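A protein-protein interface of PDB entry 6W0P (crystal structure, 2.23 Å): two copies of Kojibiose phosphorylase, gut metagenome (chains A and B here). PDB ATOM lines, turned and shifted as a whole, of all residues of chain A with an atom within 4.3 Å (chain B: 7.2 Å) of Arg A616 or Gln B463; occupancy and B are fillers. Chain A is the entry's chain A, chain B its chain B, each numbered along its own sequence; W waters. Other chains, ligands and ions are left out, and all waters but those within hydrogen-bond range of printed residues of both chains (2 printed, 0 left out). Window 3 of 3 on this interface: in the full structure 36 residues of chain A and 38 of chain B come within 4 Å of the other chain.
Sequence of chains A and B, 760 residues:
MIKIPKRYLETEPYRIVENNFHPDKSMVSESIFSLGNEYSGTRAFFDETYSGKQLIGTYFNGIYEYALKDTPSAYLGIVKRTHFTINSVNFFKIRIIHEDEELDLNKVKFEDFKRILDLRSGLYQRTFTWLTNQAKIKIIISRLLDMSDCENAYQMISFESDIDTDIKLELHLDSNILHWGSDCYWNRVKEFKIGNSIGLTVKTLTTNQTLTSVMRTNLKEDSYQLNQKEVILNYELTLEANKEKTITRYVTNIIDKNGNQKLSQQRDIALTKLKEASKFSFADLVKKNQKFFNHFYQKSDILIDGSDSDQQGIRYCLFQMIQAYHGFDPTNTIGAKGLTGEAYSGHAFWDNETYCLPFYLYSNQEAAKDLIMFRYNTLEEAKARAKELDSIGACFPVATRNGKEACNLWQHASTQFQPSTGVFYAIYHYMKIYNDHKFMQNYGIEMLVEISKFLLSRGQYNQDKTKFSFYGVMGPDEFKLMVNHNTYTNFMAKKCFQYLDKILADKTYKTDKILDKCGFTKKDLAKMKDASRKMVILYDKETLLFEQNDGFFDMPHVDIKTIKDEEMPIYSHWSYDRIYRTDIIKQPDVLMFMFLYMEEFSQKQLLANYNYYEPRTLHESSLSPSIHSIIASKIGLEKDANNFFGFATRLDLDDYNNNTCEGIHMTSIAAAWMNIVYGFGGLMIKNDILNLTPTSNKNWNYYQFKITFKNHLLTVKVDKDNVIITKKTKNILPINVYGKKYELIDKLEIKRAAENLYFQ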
ATOM      1  N   PHE A 553      22.413  20.404  24.079  1.00  0.00           N
ATOM      2  CA  PHE A 553      22.498  21.538  25.046  1.00  0.00           C
ATOM      3  C   PHE A 553      23.817  22.304  24.906  1.00  0.00           C
ATOM      4  O   PHE A 553      23.796  23.529  25.111  1.00  0.00           O
ATOM      5  CB  PHE A 553      22.415  21.053  26.498  1.00  0.00           C
ATOM      6  CG  PHE A 553      21.065  20.566  26.946  1.00  0.00           C
ATOM      7  CD1 PHE A 553      19.903  21.036  26.351  1.00  0.00           C
ATOM      8  CD2 PHE A 553      20.956  19.694  28.024  1.00  0.00           C
ATOM      9  CE1 PHE A 553      18.657  20.636  26.808  1.00  0.00           C
ATOM     10  CE2 PHE A 553      19.708  19.291  28.481  1.00  0.00           C
ATOM     11  CZ  PHE A 553      18.564  19.744  27.856  1.00  0.00           C
ATOM     12  N   ASP A 554      24.909  21.596  24.585  1.00  0.00           N
ATOM     13  CA  ASP A 554      26.296  22.140  24.567  1.00  0.00           C
ATOM     14  C   ASP A 554      26.651  22.748  23.205  1.00  0.00           C
ATOM     15  O   ASP A 554      27.749  23.310  23.094  1.00  0.00           O
ATOM     16  CB  ASP A 554      27.325  21.089  25.020  1.00  0.00           C
ATOM     17  CG  ASP A 554      28.484  21.735  25.769  1.00  0.00           C
ATOM     18  OD1 ASP A 554      28.224  22.693  26.516  1.00  0.00           O
ATOM     19  OD2 ASP A 554      29.635  21.335  25.553  1.00  0.00           O
ATOM     20  N   MET A 555      25.758  22.719  22.217  1.00  0.00           N
ATOM     21  CA  MET A 555      26.054  23.236  20.849  1.00  0.00           C
ATOM     22  C   MET A 555      26.293  24.738  20.934  1.00  0.00           C
ATOM     23  O   MET A 555      25.848  25.392  21.881  1.00  0.00           O
ATOM     24  CB  MET A 555      24.917  22.964  19.861  1.00  0.00           C
ATOM     25  CG  MET A 555      24.692  21.480  19.592  1.00  0.00           C
ATOM     26  SD  MET A 555      26.042  20.622  18.710  1.00  0.00           S
ATOM     27  CE  MET A 555      25.909  21.481  17.142  1.00  0.00           C
ATOM     28  N   PRO A 556      27.020  25.318  19.946  1.00  0.00           N
ATOM     29  CA  PRO A 556      27.139  26.764  19.818  1.00  0.00           C
ATOM     30  C   PRO A 556      25.755  27.417  19.820  1.00  0.00           C
ATOM     31  O   PRO A 556      24.852  26.925  19.134  1.00  0.00           O
ATOM     32  CB  PRO A 556      27.868  26.948  18.481  1.00  0.00           C
ATOM     33  CG  PRO A 556      28.681  25.693  18.349  1.00  0.00           C
ATOM     34  CD  PRO A 556      27.815  24.607  18.944  1.00  0.00           C
ATOM     35  N   HIS A 557      25.628  28.492  20.593  1.00  0.00           N
ATOM     36  CA  HIS A 557      24.367  29.259  20.745  1.00  0.00           C
ATOM     37  C   HIS A 557      24.293  30.313  19.646  1.00  0.00           C
ATOM     38  O   HIS A 557      25.259  31.080  19.518  1.00  0.00           O
ATOM     39  CB  HIS A 557      24.263  29.919  22.132  1.00  0.00           C
ATOM     40  CG  HIS A 557      22.980  30.665  22.272  1.00  0.00           C
ATOM     41  ND1 HIS A 557      21.740  30.023  22.175  1.00  0.00           N
ATOM     42  CD2 HIS A 557      22.721  31.985  22.429  1.00  0.00           C
ATOM     43  CE1 HIS A 557      20.784  30.932  22.299  1.00  0.00           C
ATOM     44  NE2 HIS A 557      21.360  32.137  22.457  1.00  0.00           N
ATOM     45  N   ILE A 560      18.296  33.615  17.532  1.00  0.00           N
ATOM     46  CA  ILE A 560      17.516  33.772  16.275  1.00  0.00           C
ATOM     47  C   ILE A 560      17.212  35.263  16.014  1.00  0.00           C
ATOM     48  O   ILE A 560      17.075  35.625  14.825  1.00  0.00           O
ATOM     49  CB  ILE A 560      16.249  32.906  16.347  1.00  0.00           C
ATOM     50  CG1 ILE A 560      16.622  31.432  16.205  1.00  0.00           C
ATOM     51  CG2 ILE A 560      15.241  33.345  15.298  1.00  0.00           C
ATOM     52  CD1 ILE A 560      15.468  30.492  16.392  1.00  0.00           C
ATOM     53  N   ASP A 583      22.242  25.786  17.644  1.00  0.00           N
ATOM     54  CA  ASP A 583      21.110  25.347  18.494  1.00  0.00           C
ATOM     55  C   ASP A 583      19.824  25.988  17.963  1.00  0.00           C
ATOM     56  O   ASP A 583      18.884  26.197  18.744  1.00  0.00           O
ATOM     57  CB  ASP A 583      21.426  25.653  19.953  1.00  0.00           C
ATOM     58  CG  ASP A 583      21.405  27.124  20.309  1.00  0.00           C
ATOM     59  OD1 ASP A 583      21.419  27.968  19.373  1.00  0.00           O
ATOM     60  OD2 ASP A 583      21.365  27.399  21.510  1.00  0.00           O
ATOM     61  N   ILE A 584      19.805  26.325  16.677  1.00  0.00           N
ATOM     62  CA  ILE A 584      18.604  26.834  15.963  1.00  0.00           C
ATOM     63  C   ILE A 584      17.834  25.604  15.493  1.00  0.00           C
ATOM     64  O   ILE A 584      18.449  24.730  14.853  1.00  0.00           O
ATOM     65  CB  ILE A 584      19.004  27.725  14.777  1.00  0.00           C
ATOM     66  CG1 ILE A 584      19.834  28.940  15.200  1.00  0.00           C
ATOM     67  CG2 ILE A 584      17.777  28.135  13.996  1.00  0.00           C
ATOM     68  CD1 ILE A 584      20.617  29.541  14.072  1.00  0.00           C
ATOM     69  N   ILE A 585      16.532  25.576  15.766  1.00  0.00           N
ATOM     70  CA  ILE A 585      15.616  24.433  15.525  1.00  0.00           C
ATOM     71  C   ILE A 585      14.602  24.838  14.453  1.00  0.00           C
ATOM     72  O   ILE A 585      14.096  26.003  14.472  1.00  0.00           O
ATOM     73  CB  ILE A 585      14.952  24.024  16.846  1.00  0.00           C
ATOM     74  CG1 ILE A 585      15.969  23.420  17.813  1.00  0.00           C
ATOM     75  CG2 ILE A 585      13.789  23.080  16.631  1.00  0.00           C
ATOM     76  CD1 ILE A 585      15.555  23.570  19.256  1.00  0.00           C
ATOM     77  N   TYR A 612      12.680  26.523  27.025  1.00  0.00           N
ATOM     78  CA  TYR A 612      14.010  26.214  26.437  1.00  0.00           C
ATOM     79  C   TYR A 612      13.934  26.188  24.893  1.00  0.00           C
ATOM     80  O   TYR A 612      14.808  26.789  24.270  1.00  0.00           O
ATOM     81  CB  TYR A 612      14.601  24.916  26.985  1.00  0.00           C
ATOM     82  CG  TYR A 612      16.017  24.717  26.517  1.00  0.00           C
ATOM     83  CD1 TYR A 612      17.090  25.246  27.210  1.00  0.00           C
ATOM     84  CD2 TYR A 612      16.270  24.071  25.314  1.00  0.00           C
ATOM     85  CE1 TYR A 612      18.387  25.095  26.742  1.00  0.00           C
ATOM     86  CE2 TYR A 612      17.555  23.888  24.848  1.00  0.00           C
ATOM     87  CZ  TYR A 612      18.619  24.390  25.568  1.00  0.00           C
ATOM     88  OH  TYR A 612      19.868  24.246  25.050  1.00  0.00           O
ATOM     89  N   TYR A 613      12.932  25.540  24.292  1.00  0.00           N
ATOM     90  CA  TYR A 613      12.909  25.210  22.840  1.00  0.00           C
ATOM     91  C   TYR A 613      12.194  26.257  21.980  1.00  0.00           C
ATOM     92  O   TYR A 613      12.685  26.476  20.860  1.00  0.00           O
ATOM     93  CB  TYR A 613      12.360  23.803  22.639  1.00  0.00           C
ATOM     94  CG  TYR A 613      13.336  22.738  23.072  1.00  0.00           C
ATOM     95  CD1 TYR A 613      14.541  22.555  22.418  1.00  0.00           C
ATOM     96  CD2 TYR A 613      13.066  21.925  24.153  1.00  0.00           C
ATOM     97  CE1 TYR A 613      15.446  21.590  22.831  1.00  0.00           C
ATOM     98  CE2 TYR A 613      13.950  20.947  24.563  1.00  0.00           C
ATOM     99  CZ  TYR A 613      15.151  20.787  23.911  1.00  0.00           C
ATOM    100  OH  TYR A 613      16.006  19.824  24.348  1.00  0.00           O
ATOM    101  N   GLU A 614      11.093  26.863  22.436  1.00  0.00           N
ATOM    102  CA  GLU A 614      10.369  27.882  21.633  1.00  0.00           C
ATOM    103  C   GLU A 614      11.341  28.978  21.168  1.00  0.00           C
ATOM    104  O   GLU A 614      11.348  29.286  19.987  1.00  0.00           O
ATOM    105  CB  GLU A 614       9.166  28.453  22.394  1.00  0.00           C
ATOM    106  CG  GLU A 614       8.329  29.448  21.595  1.00  0.00           C
ATOM    107  CD  GLU A 614       8.969  30.791  21.257  1.00  0.00           C
ATOM    108  OE1 GLU A 614       9.481  31.426  22.175  1.00  0.00           O
ATOM    109  OE2 GLU A 614       8.986  31.178  20.023  1.00  0.00           O
ATOM    110  N   PRO A 615      12.172  29.628  22.027  1.00  0.00           N
ATOM    111  CA  PRO A 615      13.054  30.713  21.558  1.00  0.00           C
ATOM    112  C   PRO A 615      14.272  30.304  20.697  1.00  0.00           C
ATOM    113  O   PRO A 615      14.891  31.176  20.082  1.00  0.00           O
ATOM    114  CB  PRO A 615      13.539  31.408  22.844  1.00  0.00           C
ATOM    115  CG  PRO A 615      13.340  30.384  23.952  1.00  0.00           C
ATOM    116  CD  PRO A 615      12.220  29.460  23.491  1.00  0.00           C
ATOM    117  N   ARG A 616      14.578  29.002  20.630  1.00  0.00           N
ATOM    118  CA  ARG A 616      15.569  28.434  19.682  1.00  0.00           C
ATOM    119  C   ARG A 616      14.909  27.994  18.368  1.00  0.00           C
ATOM    120  O   ARG A 616      15.651  27.514  17.488  1.00  0.00           O
ATOM    121  CB  ARG A 616      16.278  27.253  20.339  1.00  0.00           C
ATOM    122  CG  ARG A 616      17.049  27.651  21.587  1.00  0.00           C
ATOM    123  CD  ARG A 616      17.833  26.513  22.195  1.00  0.00           C
ATOM    124  NE  ARG A 616      18.900  27.019  23.046  1.00  0.00           N
ATOM    125  CZ  ARG A 616      18.718  27.496  24.279  1.00  0.00           C
ATOM    126  NH1 ARG A 616      17.503  27.554  24.805  1.00  0.00           N
ATOM    127  NH2 ARG A 616      19.755  27.917  24.982  1.00  0.00           N
ATOM    128  N   THR A 617      13.589  28.126  18.217  1.00  0.00           N
ATOM    129  CA  THR A 617      12.838  27.547  17.070  1.00  0.00           C
ATOM    130  C   THR A 617      12.551  28.644  16.029  1.00  0.00           C
ATOM    131  O   THR A 617      11.928  29.665  16.354  1.00  0.00           O
ATOM    132  CB  THR A 617      11.570  26.838  17.522  1.00  0.00           C
ATOM    133  OG1 THR A 617      11.952  25.872  18.495  1.00  0.00           O
ATOM    134  CG2 THR A 617      10.863  26.180  16.359  1.00  0.00           C
ATOM    135  N   LEU A 618      13.031  28.428  14.806  1.00  0.00           N
ATOM    136  CA  LEU A 618      12.909  29.395  13.686  1.00  0.00           C
ATOM    137  C   LEU A 618      11.458  29.448  13.222  1.00  0.00           C
ATOM    138  O   LEU A 618      11.038  30.514  12.785  1.00  0.00           O
ATOM    139  CB  LEU A 618      13.859  28.940  12.577  1.00  0.00           C
ATOM    140  CG  LEU A 618      14.359  30.002  11.615  1.00  0.00           C
ATOM    141  CD1 LEU A 618      15.080  31.114  12.331  1.00  0.00           C
ATOM    142  CD2 LEU A 618      15.282  29.352  10.594  1.00  0.00           C
ATOM    143  N   TYR B 461      32.992  28.334  19.779  1.00  0.00           N
ATOM    144  CA  TYR B 461      32.784  28.100  21.220  1.00  0.00           C
ATOM    145  C   TYR B 461      31.471  27.330  21.380  1.00  0.00           C
ATOM    146  O   TYR B 461      30.532  27.511  20.590  1.00  0.00           O
ATOM    147  CB  TYR B 461      32.794  29.424  21.982  1.00  0.00           C
ATOM    148  CG  TYR B 461      34.123  30.138  22.022  1.00  0.00           C
ATOM    149  CD1 TYR B 461      35.099  29.775  22.936  1.00  0.00           C
ATOM    150  CD2 TYR B 461      34.378  31.224  21.199  1.00  0.00           C
ATOM    151  CE1 TYR B 461      36.307  30.453  23.010  1.00  0.00           C
ATOM    152  CE2 TYR B 461      35.575  31.925  21.267  1.00  0.00           C
ATOM    153  CZ  TYR B 461      36.547  31.529  22.172  1.00  0.00           C
ATOM    154  OH  TYR B 461      37.748  32.176  22.225  1.00  0.00           O
ATOM    155  N   ASN B 462      31.420  26.479  22.392  1.00  0.00           N
ATOM    156  CA  ASN B 462      30.204  25.764  22.837  1.00  0.00           C
ATOM    157  C   ASN B 462      29.195  26.767  23.420  1.00  0.00           C
ATOM    158  O   ASN B 462      29.468  27.986  23.417  1.00  0.00           O
ATOM    159  CB  ASN B 462      30.597  24.649  23.810  1.00  0.00           C
ATOM    160  CG  ASN B 462      30.965  25.160  25.188  1.00  0.00           C
ATOM    161  OD1 ASN B 462      31.613  26.191  25.320  1.00  0.00           O
ATOM    162  ND2 ASN B 462      30.532  24.461  26.218  1.00  0.00           N
ATOM    163  N   GLN B 463      28.077  26.244  23.935  1.00  0.00           N
ATOM    164  CA  GLN B 463      26.880  26.980  24.425  1.00  0.00           C
ATOM    165  C   GLN B 463      27.320  28.071  25.421  1.00  0.00           C
ATOM    166  O   GLN B 463      26.928  29.224  25.220  1.00  0.00           O
ATOM    167  CB  GLN B 463      25.859  25.986  25.006  1.00  0.00           C
ATOM    168  CG  GLN B 463      24.532  26.620  25.446  1.00  0.00           C
ATOM    169  CD  GLN B 463      23.500  26.921  24.371  1.00  0.00           C
ATOM    170  OE1 GLN B 463      22.559  27.684  24.595  1.00  0.00           O
ATOM    171  NE2 GLN B 463      23.606  26.284  23.216  1.00  0.00           N
ATOM    172  N   ASP B 464      28.118  27.735  26.436  1.00  0.00           N
ATOM    173  CA  ASP B 464      28.516  28.671  27.530  1.00  0.00           C
ATOM    174  C   ASP B 464      29.917  29.265  27.274  1.00  0.00           C
ATOM    175  O   ASP B 464      30.385  30.008  28.123  1.00  0.00           O
ATOM    176  CB  ASP B 464      28.425  27.979  28.896  1.00  0.00           C
ATOM    177  CG  ASP B 464      29.422  26.854  29.131  1.00  0.00           C
ATOM    178  OD1 ASP B 464      30.334  26.707  28.310  1.00  0.00           O
ATOM    179  OD2 ASP B 464      29.289  26.135  30.155  1.00  0.00           O
ATOM    180  N   LYS B 465      30.590  28.915  26.172  1.00  0.00           N
ATOM    181  CA  LYS B 465      31.856  29.555  25.720  1.00  0.00           C
ATOM    182  C   LYS B 465      33.037  29.192  26.632  1.00  0.00           C
ATOM    183  O   LYS B 465      34.051  29.909  26.601  1.00  0.00           O
ATOM    184  CB  LYS B 465      31.656  31.071  25.606  1.00  0.00           C
ATOM    185  CG  LYS B 465      30.509  31.484  24.691  1.00  0.00           C
ATOM    186  CD  LYS B 465      30.653  32.874  24.106  1.00  0.00           C
ATOM    187  CE  LYS B 465      29.838  33.081  22.844  1.00  0.00           C
ATOM    188  NZ  LYS B 465      30.471  34.086  21.950  1.00  0.00           N
ATOM    189  N   THR B 466      32.951  28.075  27.354  1.00  0.00           N
ATOM    190  CA  THR B 466      34.071  27.530  28.159  1.00  0.00           C
ATOM    191  C   THR B 466      34.950  26.632  27.288  1.00  0.00           C
ATOM    192  O   THR B 466      36.085  26.375  27.671  1.00  0.00           O
ATOM    193  CB  THR B 466      33.537  26.775  29.379  1.00  0.00           C
ATOM    194  OG1 THR B 466      32.634  25.771  28.916  1.00  0.00           O
ATOM    195  CG2 THR B 466      32.834  27.704  30.345  1.00  0.00           C
ATOM    196  N   LYS B 467      34.435  26.165  26.159  1.00  0.00           N
ATOM    197  CA  LYS B 467      35.154  25.235  25.257  1.00  0.00           C
ATOM    198  C   LYS B 467      35.220  25.801  23.837  1.00  0.00           C
ATOM    199  O   LYS B 467      34.302  26.516  23.427  1.00  0.00           O
ATOM    200  CB  LYS B 467      34.431  23.892  25.190  1.00  0.00           C
ATOM    201  CG  LYS B 467      34.170  23.225  26.523  1.00  0.00           C
ATOM    202  CD  LYS B 467      33.365  21.952  26.341  1.00  0.00           C
ATOM    203  CE  LYS B 467      32.679  21.482  27.608  1.00  0.00           C
ATOM    204  NZ  LYS B 467      31.715  20.407  27.274  1.00  0.00           N
ATOM    205  N   TYR B 471      32.515  21.761  15.177  1.00  0.00           N
ATOM    206  CA  TYR B 471      31.204  21.084  15.119  1.00  0.00           C
ATOM    207  C   TYR B 471      30.885  20.797  13.655  1.00  0.00           C
ATOM    208  O   TYR B 471      31.260  21.625  12.753  1.00  0.00           O
ATOM    209  CB  TYR B 471      30.150  21.954  15.808  1.00  0.00           C
ATOM    210  CG  TYR B 471      30.355  22.129  17.290  1.00  0.00           C
ATOM    211  CD1 TYR B 471      31.184  23.126  17.773  1.00  0.00           C
ATOM    212  CD2 TYR B 471      29.719  21.311  18.209  1.00  0.00           C
ATOM    213  CE1 TYR B 471      31.369  23.323  19.131  1.00  0.00           C
ATOM    214  CE2 TYR B 471      29.894  21.494  19.569  1.00  0.00           C
ATOM    215  CZ  TYR B 471      30.732  22.499  20.031  1.00  0.00           C
ATOM    216  OH  TYR B 471      30.951  22.694  21.367  1.00  0.00           O
HETATM  217  O   HOH W   1      29.994  20.685  22.822  1.00  0.00           O
HETATM  218  O   HOH W   2      27.797  29.722  22.147  1.00  0.00           O
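Of the printed residues of chain B, Pro A556 touches Tyr B461 (3.4 Å) and Tyr B471 (3.6 Å). Of the printed residues of chain B, His A557 touches Gln B463. Printed residues of chain B within 4 Å of Asp A583: Gln B463. Of chain B, only Gln B463 (2.8 Å) comes within 4 Å of Arg A616. Of the printed residues of chain A, Tyr B461 touches Pro A556 (3.4 Å). Gln B463 touches just these residues of chain A: Phe A553, Asp A554, Met A555, His A557, Asp A583 and Arg A616. Lys B465 touches none of the printed residues of chain A. Of the printed residues of chain A, Lys B467 touches Asp A554 (2.9 Å). The nearest printed residue of chain B that does not touch Arg A616 is Asp B464 (8.5 Å).
The backbone carbonyl oxygen (O) of Pro A556 sits at hydrogen-bond distance from the backbone NH (N) of Asp A583 (3.2 Å). ND1 of His A557 is in hydrogen-bond range of OD2 of Asp A583 (2.7 Å). The backbone NH (N) of Ile A585 lies within hydrogen-bond range of the backbone carbonyl oxygen (O) of Arg A616 (2.7 Å). The side-chain amide nitrogen of Asn B462 sits at hydrogen-bond distance from the side-chain carboxylate of Asp B464 (3.1 Å). OD1 of Asn B462 lies within hydrogen-bond range of N of Lys B465 (3.0 Å). The backbone NH (N) of Thr B466 is in hydrogen-bond range of the side-chain amide oxygen (OD1) of Asn B462 (3.1 Å).
Asp A554 touches Tyr B471. O of Met A555 touches C of Asn B462 (3.9 Å). Met A555 touches Tyr B471 (SD to CD2, 3.8 Å). CG of Pro A556 touches O of Tyr B461, at 3.4 Å. CD1 of Tyr B471 touches CG of Pro A556 (3.6 Å).
Of the 16 printed residues of chain A, 7 touch a printed residue of chain B. Printed residues of chain A that touch a printed residue of chain B: Phe A553, Asp A554, Met A555, Pro A556, His A557, Asp A583 and Arg A616. Hydrophobic or aromatic side chains of chain B that line the printed part of chain A: Tyr B471.
No position is printed for both chains.
Water W1 lies within hydrogen-bond range of the side-chain hydroxyl (OH) of Tyr B471 and the side-chain carboxylate (OD2) of Asp A554. Water W2 lies within hydrogen-bond range of the backbone carbonyl oxygen (O) of Asn B462 (2.7 Å), the backbone NH (N) of His A557 (2.9 Å) and the backbone carbonyl oxygen (O) of Gln B463 (3.2 Å).
O of Phe A553 lies close to NE2 of Gln B463 (3.3 Å). The side-chain carboxylate (OD1) of Asp A554 sits at hydrogen-bond distance from the side-chain amide nitrogen (ND2) of Asn B462 (2.9 Å). The backbone NH (N) of Gln B463 is in hydrogen-bond range of the backbone carbonyl oxygen (O) of Asp A554, 3.1 Å away. NZ of Lys B467 lies within salt-bridge range of OD2 of Asp A554, 2.9 Å away. The backbone carbonyl oxygen (O) of Met A555 lies within hydrogen-bond range of the side-chain amide nitrogen (NE2) of Gln B463, 2.8 Å away. OE1 of Gln B463 lies within hydrogen-bond range of ND1 of His A557. The side-chain carboxylate of Asp A583 lies within hydrogen-bond range of the side-chain amide nitrogen of Gln B463 (3.0 Å). The guanidinium group of Arg A616 sits at hydrogen-bond distance from the side-chain amide oxygen of Gln B463 (2.8 Å).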
